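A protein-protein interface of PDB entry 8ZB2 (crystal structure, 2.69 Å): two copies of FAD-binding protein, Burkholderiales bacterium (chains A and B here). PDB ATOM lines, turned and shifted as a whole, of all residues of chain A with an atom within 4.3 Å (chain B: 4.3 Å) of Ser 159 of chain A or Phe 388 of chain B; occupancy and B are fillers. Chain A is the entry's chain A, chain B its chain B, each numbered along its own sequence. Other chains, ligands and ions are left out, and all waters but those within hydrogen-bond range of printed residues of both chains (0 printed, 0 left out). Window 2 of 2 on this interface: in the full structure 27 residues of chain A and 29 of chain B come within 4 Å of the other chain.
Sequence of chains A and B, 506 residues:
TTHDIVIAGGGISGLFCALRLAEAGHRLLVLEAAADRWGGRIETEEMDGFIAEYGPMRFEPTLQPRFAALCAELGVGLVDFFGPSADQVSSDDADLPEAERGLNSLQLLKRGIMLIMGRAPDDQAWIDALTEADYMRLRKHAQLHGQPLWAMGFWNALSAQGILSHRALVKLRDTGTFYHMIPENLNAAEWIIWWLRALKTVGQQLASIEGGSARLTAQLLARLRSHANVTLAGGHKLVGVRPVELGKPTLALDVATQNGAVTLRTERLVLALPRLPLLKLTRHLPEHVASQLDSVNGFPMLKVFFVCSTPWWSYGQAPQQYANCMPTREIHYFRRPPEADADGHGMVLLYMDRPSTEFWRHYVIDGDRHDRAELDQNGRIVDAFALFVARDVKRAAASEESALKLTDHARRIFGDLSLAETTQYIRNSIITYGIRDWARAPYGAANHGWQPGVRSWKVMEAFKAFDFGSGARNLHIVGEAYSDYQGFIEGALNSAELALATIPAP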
ATOM      1  N   TRP A 155     -26.221   4.579  17.718  1.00  0.00           N
ATOM      2  CA  TRP A 155     -26.453   5.869  17.030  1.00  0.00           C
ATOM      3  C   TRP A 155     -27.068   6.859  18.013  1.00  0.00           C
ATOM      4  O   TRP A 155     -26.669   8.032  17.994  1.00  0.00           O
ATOM      5  CB  TRP A 155     -27.347   5.639  15.827  1.00  0.00           C
ATOM      6  CG  TRP A 155     -27.523   6.840  14.961  1.00  0.00           C
ATOM      7  CD1 TRP A 155     -27.089   8.115  15.187  1.00  0.00           C
ATOM      8  CD2 TRP A 155     -28.264   6.873  13.726  1.00  0.00           C
ATOM      9  NE1 TRP A 155     -27.510   8.938  14.176  1.00  0.00           N
ATOM     10  CE2 TRP A 155     -28.237   8.208  13.269  1.00  0.00           C
ATOM     11  CE3 TRP A 155     -28.955   5.911  12.979  1.00  0.00           C
ATOM     12  CZ2 TRP A 155     -28.862   8.594  12.086  1.00  0.00           C
ATOM     13  CZ3 TRP A 155     -29.574   6.292  11.815  1.00  0.00           C
ATOM     14  CH2 TRP A 155     -29.512   7.613  11.372  1.00  0.00           C
ATOM     15  N   ASN A 156     -27.980   6.395  18.869  1.00  0.00           N
ATOM     16  CA  ASN A 156     -28.698   7.281  19.819  1.00  0.00           C
ATOM     17  C   ASN A 156     -27.704   7.724  20.895  1.00  0.00           C
ATOM     18  O   ASN A 156     -27.669   8.933  21.198  1.00  0.00           O
ATOM     19  CB  ASN A 156     -29.959   6.626  20.407  1.00  0.00           C
ATOM     20  CG  ASN A 156     -30.947   6.140  19.361  1.00  0.00           C
ATOM     21  OD1 ASN A 156     -30.757   5.079  18.772  1.00  0.00           O
ATOM     22  ND2 ASN A 156     -32.012   6.883  19.122  1.00  0.00           N
ATOM     23  N   ALA A 157     -26.947   6.796  21.476  1.00  0.00           N
ATOM     24  CA  ALA A 157     -25.984   7.085  22.575  1.00  0.00           C
ATOM     25  C   ALA A 157     -24.971   8.141  22.107  1.00  0.00           C
ATOM     26  O   ALA A 157     -24.701   9.072  22.877  1.00  0.00           O
ATOM     27  CB  ALA A 157     -25.288   5.826  23.038  1.00  0.00           C
ATOM     28  N   LEU A 158     -24.475   8.026  20.869  1.00  0.00           N
ATOM     29  CA  LEU A 158     -23.522   9.002  20.270  1.00  0.00           C
ATOM     30  C   LEU A 158     -24.203  10.368  20.026  1.00  0.00           C
ATOM     31  O   LEU A 158     -23.476  11.343  19.934  1.00  0.00           O
ATOM     32  CB  LEU A 158     -22.937   8.454  18.959  1.00  0.00           C
ATOM     33  CG  LEU A 158     -21.991   7.248  19.040  1.00  0.00           C
ATOM     34  CD1 LEU A 158     -21.447   6.912  17.656  1.00  0.00           C
ATOM     35  CD2 LEU A 158     -20.848   7.460  20.030  1.00  0.00           C
ATOM     36  N   SER A 159     -25.527  10.454  19.898  1.00  0.00           N
ATOM     37  CA  SER A 159     -26.251  11.697  19.511  1.00  0.00           C
ATOM     38  C   SER A 159     -26.783  12.379  20.762  1.00  0.00           C
ATOM     39  O   SER A 159     -27.566  13.347  20.646  1.00  0.00           O
ATOM     40  CB  SER A 159     -27.403  11.418  18.591  1.00  0.00           C
ATOM     41  OG  SER A 159     -26.989  10.775  17.405  1.00  0.00           O
ATOM     42  N   ALA A 160     -26.438  11.850  21.931  1.00  0.00           N
ATOM     43  CA  ALA A 160     -27.035  12.283  23.212  1.00  0.00           C
ATOM     44  C   ALA A 160     -26.559  13.692  23.583  1.00  0.00           C
ATOM     45  O   ALA A 160     -25.563  14.171  23.006  1.00  0.00           O
ATOM     46  CB  ALA A 160     -26.690  11.285  24.281  1.00  0.00           C
ATOM     47  N   GLN A 161     -27.252  14.321  24.528  1.00  0.00           N
ATOM     48  CA  GLN A 161     -26.822  15.561  25.223  1.00  0.00           C
ATOM     49  C   GLN A 161     -25.389  15.338  25.723  1.00  0.00           C
ATOM     50  O   GLN A 161     -25.175  14.403  26.550  1.00  0.00           O
ATOM     51  CB  GLN A 161     -27.805  15.872  26.355  1.00  0.00           C
ATOM     52  CG  GLN A 161     -27.717  17.282  26.915  1.00  0.00           C
ATOM     53  CD  GLN A 161     -26.608  17.442  27.933  1.00  0.00           C
ATOM     54  OE1 GLN A 161     -26.544  16.728  28.938  1.00  0.00           O
ATOM     55  NE2 GLN A 161     -25.730  18.403  27.685  1.00  0.00           N
ATOM     56  N   LEU A 164     -21.961  13.795  20.622  1.00  0.00           N
ATOM     57  CA  LEU A 164     -21.580  14.216  19.247  1.00  0.00           C
ATOM     58  C   LEU A 164     -22.747  14.895  18.522  1.00  0.00           C
ATOM     59  O   LEU A 164     -23.892  14.797  18.975  1.00  0.00           O
ATOM     60  CB  LEU A 164     -21.122  13.012  18.411  1.00  0.00           C
ATOM     61  CG  LEU A 164     -19.932  12.189  18.917  1.00  0.00           C
ATOM     62  CD1 LEU A 164     -19.345  11.369  17.783  1.00  0.00           C
ATOM     63  CD2 LEU A 164     -18.853  13.049  19.543  1.00  0.00           C
ATOM     64  N   LYS A 171     -21.466  15.849  11.285  1.00  0.00           N
ATOM     65  CA  LYS A 171     -21.910  15.673  12.692  1.00  0.00           C
ATOM     66  C   LYS A 171     -21.397  14.318  13.179  1.00  0.00           C
ATOM     67  O   LYS A 171     -20.242  14.279  13.598  1.00  0.00           O
ATOM     68  CB  LYS A 171     -23.436  15.701  12.815  1.00  0.00           C
ATOM     69  CG  LYS A 171     -24.158  16.873  12.176  1.00  0.00           C
ATOM     70  CD  LYS A 171     -25.656  16.797  12.451  1.00  0.00           C
ATOM     71  CE  LYS A 171     -26.202  15.381  12.571  1.00  0.00           C
ATOM     72  NZ  LYS A 171     -27.383  15.311  13.462  1.00  0.00           N
ATOM     73  N   LEU A 172     -22.256  13.282  13.151  1.00  0.00           N
ATOM     74  CA  LEU A 172     -21.885  11.846  13.046  1.00  0.00           C
ATOM     75  C   LEU A 172     -21.584  11.522  11.578  1.00  0.00           C
ATOM     76  O   LEU A 172     -22.550  11.556  10.787  1.00  0.00           O
ATOM     77  CB  LEU A 172     -23.044  10.966  13.531  1.00  0.00           C
ATOM     78  CG  LEU A 172     -23.156  10.783  15.044  1.00  0.00           C
ATOM     79  CD1 LEU A 172     -24.089  11.819  15.635  1.00  0.00           C
ATOM     80  CD2 LEU A 172     -23.628   9.383  15.402  1.00  0.00           C
ATOM     81  N   CYS B 325     -28.808  16.685   9.110  1.00  0.00           N
ATOM     82  CA  CYS B 325     -29.030  17.709  10.184  1.00  0.00           C
ATOM     83  C   CYS B 325     -29.871  17.127  11.333  1.00  0.00           C
ATOM     84  O   CYS B 325     -29.565  17.397  12.512  1.00  0.00           O
ATOM     85  CB  CYS B 325     -29.735  18.948   9.638  1.00  0.00           C
ATOM     86  SG  CYS B 325     -30.968  19.640  10.775  1.00  0.00           S
ATOM     87  N   MET B 326     -30.918  16.384  10.975  1.00  0.00           N
ATOM     88  CA  MET B 326     -31.695  15.474  11.859  1.00  0.00           C
ATOM     89  C   MET B 326     -31.638  14.070  11.268  1.00  0.00           C
ATOM     90  O   MET B 326     -31.594  13.890  10.049  1.00  0.00           O
ATOM     91  CB  MET B 326     -33.155  15.913  11.927  1.00  0.00           C
ATOM     92  CG  MET B 326     -33.401  16.982  12.954  1.00  0.00           C
ATOM     93  SD  MET B 326     -35.024  16.724  13.708  1.00  0.00           S
ATOM     94  CE  MET B 326     -34.800  15.081  14.386  1.00  0.00           C
ATOM     95  N   PRO B 327     -31.632  13.004  12.088  1.00  0.00           N
ATOM     96  CA  PRO B 327     -31.981  11.691  11.565  1.00  0.00           C
ATOM     97  C   PRO B 327     -33.477  11.731  11.199  1.00  0.00           C
ATOM     98  O   PRO B 327     -34.278  11.380  12.022  1.00  0.00           O
ATOM     99  CB  PRO B 327     -31.621  10.741  12.715  1.00  0.00           C
ATOM    100  CG  PRO B 327     -30.754  11.569  13.654  1.00  0.00           C
ATOM    101  CD  PRO B 327     -31.255  12.990  13.507  1.00  0.00           C
ATOM    102  N   PHE B 359     -33.022   4.879  13.790  1.00  0.00           N
ATOM    103  CA  PHE B 359     -32.718   5.810  14.911  1.00  0.00           C
ATOM    104  C   PHE B 359     -33.876   5.790  15.913  1.00  0.00           C
ATOM    105  O   PHE B 359     -33.606   5.698  17.134  1.00  0.00           O
ATOM    106  CB  PHE B 359     -32.472   7.253  14.444  1.00  0.00           C
ATOM    107  CG  PHE B 359     -32.107   8.197  15.564  1.00  0.00           C
ATOM    108  CD1 PHE B 359     -33.082   8.856  16.295  1.00  0.00           C
ATOM    109  CD2 PHE B 359     -30.783   8.393  15.917  1.00  0.00           C
ATOM    110  CE1 PHE B 359     -32.744   9.683  17.358  1.00  0.00           C
ATOM    111  CE2 PHE B 359     -30.435   9.222  16.977  1.00  0.00           C
ATOM    112  CZ  PHE B 359     -31.418   9.867  17.696  1.00  0.00           C
ATOM    113  N   ALA B 384     -34.742  14.146  22.291  1.00  0.00           N
ATOM    114  CA  ALA B 384     -33.816  13.957  21.151  1.00  0.00           C
ATOM    115  C   ALA B 384     -34.255  14.843  19.980  1.00  0.00           C
ATOM    116  O   ALA B 384     -33.399  15.331  19.258  1.00  0.00           O
ATOM    117  CB  ALA B 384     -33.724  12.498  20.790  1.00  0.00           C
ATOM    118  N   PHE B 385     -35.548  15.072  19.815  1.00  0.00           N
ATOM    119  CA  PHE B 385     -36.083  16.079  18.867  1.00  0.00           C
ATOM    120  C   PHE B 385     -35.568  17.466  19.268  1.00  0.00           C
ATOM    121  O   PHE B 385     -35.050  18.210  18.401  1.00  0.00           O
ATOM    122  CB  PHE B 385     -37.609  16.052  18.882  1.00  0.00           C
ATOM    123  CG  PHE B 385     -38.256  17.177  18.126  1.00  0.00           C
ATOM    124  CD1 PHE B 385     -38.087  17.295  16.761  1.00  0.00           C
ATOM    125  CD2 PHE B 385     -39.051  18.108  18.779  1.00  0.00           C
ATOM    126  CE1 PHE B 385     -38.710  18.321  16.063  1.00  0.00           C
ATOM    127  CE2 PHE B 385     -39.671  19.132  18.081  1.00  0.00           C
ATOM    128  CZ  PHE B 385     -39.502  19.233  16.723  1.00  0.00           C
ATOM    129  N   ALA B 386     -35.711  17.811  20.552  1.00  0.00           N
ATOM    130  CA  ALA B 386     -35.238  19.089  21.120  1.00  0.00           C
ATOM    131  C   ALA B 386     -33.793  19.329  20.658  1.00  0.00           C
ATOM    132  O   ALA B 386     -33.614  20.182  19.780  1.00  0.00           O
ATOM    133  CB  ALA B 386     -35.373  19.057  22.620  1.00  0.00           C
ATOM    134  N   LEU B 387     -32.831  18.547  21.174  1.00  0.00           N
ATOM    135  CA  LEU B 387     -31.368  18.662  20.918  1.00  0.00           C
ATOM    136  C   LEU B 387     -31.109  18.815  19.420  1.00  0.00           C
ATOM    137  O   LEU B 387     -30.349  19.713  19.058  1.00  0.00           O
ATOM    138  CB  LEU B 387     -30.664  17.426  21.487  1.00  0.00           C
ATOM    139  CG  LEU B 387     -29.131  17.359  21.421  1.00  0.00           C
ATOM    140  CD1 LEU B 387     -28.654  16.704  20.129  1.00  0.00           C
ATOM    141  CD2 LEU B 387     -28.451  18.714  21.625  1.00  0.00           C
ATOM    142  N   PHE B 388     -31.707  17.984  18.570  1.00  0.00           N
ATOM    143  CA  PHE B 388     -31.431  18.012  17.112  1.00  0.00           C
ATOM    144  C   PHE B 388     -31.897  19.361  16.549  1.00  0.00           C
ATOM    145  O   PHE B 388     -31.114  19.990  15.835  1.00  0.00           O
ATOM    146  CB  PHE B 388     -32.007  16.780  16.404  1.00  0.00           C
ATOM    147  CG  PHE B 388     -31.161  15.535  16.556  1.00  0.00           C
ATOM    148  CD1 PHE B 388     -29.914  15.434  15.953  1.00  0.00           C
ATOM    149  CD2 PHE B 388     -31.603  14.452  17.299  1.00  0.00           C
ATOM    150  CE1 PHE B 388     -29.138  14.289  16.090  1.00  0.00           C
ATOM    151  CE2 PHE B 388     -30.825  13.316  17.443  1.00  0.00           C
ATOM    152  CZ  PHE B 388     -29.593  13.238  16.841  1.00  0.00           C
ATOM    153  N   VAL B 389     -33.099  19.824  16.877  1.00  0.00           N
ATOM    154  CA  VAL B 389     -33.603  21.140  16.367  1.00  0.00           C
ATOM    155  C   VAL B 389     -32.816  22.287  17.041  1.00  0.00           C
ATOM    156  O   VAL B 389     -32.358  23.181  16.308  1.00  0.00           O
ATOM    157  CB  VAL B 389     -35.131  21.277  16.523  1.00  0.00           C
ATOM    158  CG1 VAL B 389     -35.600  22.722  16.417  1.00  0.00           C
ATOM    159  CG2 VAL B 389     -35.862  20.420  15.497  1.00  0.00           C
ATOM    160  N   ALA B 390     -32.613  22.229  18.362  1.00  0.00           N
ATOM    161  CA  ALA B 390     -31.870  23.224  19.181  1.00  0.00           C
ATOM    162  C   ALA B 390     -30.564  23.652  18.489  1.00  0.00           C
ATOM    163  O   ALA B 390     -30.335  24.860  18.378  1.00  0.00           O
ATOM    164  CB  ALA B 390     -31.596  22.681  20.570  1.00  0.00           C
ATOM    165  N   ARG B 391     -29.733  22.697  18.059  1.00  0.00           N
ATOM    166  CA  ARG B 391     -28.542  22.951  17.201  1.00  0.00           C
ATOM    167  C   ARG B 391     -28.969  23.803  16.003  1.00  0.00           C
ATOM    168  O   ARG B 391     -28.463  24.935  15.872  1.00  0.00           O
ATOM    169  CB  ARG B 391     -27.926  21.657  16.657  1.00  0.00           C
ATOM    170  CG  ARG B 391     -27.294  20.763  17.703  1.00  0.00           C
ATOM    171  CD  ARG B 391     -26.460  19.683  17.047  1.00  0.00           C
ATOM    172  NE  ARG B 391     -26.254  18.580  17.972  1.00  0.00           N
ATOM    173  CZ  ARG B 391     -25.467  18.617  19.052  1.00  0.00           C
ATOM    174  NH1 ARG B 391     -24.790  19.712  19.371  1.00  0.00           N
ATOM    175  NH2 ARG B 391     -25.378  17.546  19.823  1.00  0.00           N
ATOM    176  N   ASP B 392     -29.894  23.288  15.189  1.00  0.00           N
ATOM    177  CA  ASP B 392     -30.231  23.853  13.858  1.00  0.00           C
ATOM    178  C   ASP B 392     -30.828  25.263  13.991  1.00  0.00           C
ATOM    179  O   ASP B 392     -30.720  26.016  13.008  1.00  0.00           O
ATOM    180  CB  ASP B 392     -31.176  22.937  13.080  1.00  0.00           C
ATOM    181  CG  ASP B 392     -31.502  23.449  11.684  1.00  0.00           C
ATOM    182  OD1 ASP B 392     -32.416  24.293  11.567  1.00  0.00           O
ATOM    183  OD2 ASP B 392     -30.837  23.008  10.725  1.00  0.00           O
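The backbone carbonyl oxygen (O) of Trp 155 of chain A is in hydrogen-bond range of the side-chain hydroxyl (OG) of Ser 159 of chain A, 2.8 Å away. The backbone carbonyl oxygen of Leu 158 of chain A lies within hydrogen-bond range of the backbone NH of Leu 164 of chain A (3.0 Å). The side-chain sulfur (SG) of Cys 325 of chain B is in hydrogen-bond range of the side-chain carboxylate (OD2) of Asp 392 of chain B (3.4 Å).
CB of Pro 327 of chain B touches CZ2 of Trp 155 of chain A, 3.6 Å away. Phe 359 of chain B touches Trp 155 of chain A. Phe 359 of chain B touches Ser 159 of chain A (CE2 to OG, 3.8 Å). Ser 159 of chain A touches Leu 387 of chain B. CB of Ser 159 of chain A touches CZ of Phe 388 of chain B (3.3 Å). Lys 171 of chain A touches Phe 388 of chain B (NZ to CE1, 3.3 Å).
Ser 159 of chain A touches just these residues of chain B: Phe 359 (3.8 Å), Leu 387 (3.6 Å) and Phe 388 (3.3 Å). Phe 388 of chain B touches just these residues of chain A: Ser 159 (3.3 Å) and Lys 171 (3.3 Å). Of the printed residues of chain B, Leu 164 of chain A touches Arg 391 (3.2 Å). Of the printed residues of chain A, Leu 387 of chain B touches Ser 159 (3.6 Å). The nearest printed residue of chain B that does not touch Ser 159 of chain A is Arg 391 of chain B (4.8 Å). The nearest printed residue of chain A that does not touch Phe 388 of chain B is Trp 155 of chain A (5.5 Å). The nearest printed residue of chain B that does not touch Trp 155 of chain A is Phe 388 of chain B (5.5 Å).
The side-chain amide nitrogen of Asn 156 of chain A is in hydrogen-bond range of the backbone carbonyl oxygen of Phe 359 of chain B. The guanidinium group of Arg 391 of chain B sits at hydrogen-bond distance from the backbone carbonyl oxygen of Leu 164 of chain A (3.2 Å). NZ of Lys 171 of chain A is in hydrogen-bond range of O of Cys 325 of chain B.
Printed residues of chain B that touch a printed residue of chain A: Cys 325, Pro 327, Phe 359, Leu 387, Phe 388 and Arg 391. Hydrophobic or aromatic side chains of chain B that line the printed part of chain A: Pro 327, Phe 359, Leu 387 and Phe 388. Of the 10 printed residues of chain A, 5 touch a printed residue of chain B. Hydrophobic or aromatic side chains of chain A that line the printed part of chain B: Trp 155. Among the printed residues, 9 pairs touch across the chains. Among the printed residues, no Asp or Glu carboxylate lies within 4 Å of a Lys or Arg side-chain nitrogen of the other chain.
No position is printed for both chains. Of the 9 pairs that touch across the chains among the printed residues, none has its exchanged pair printed and touching as well.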
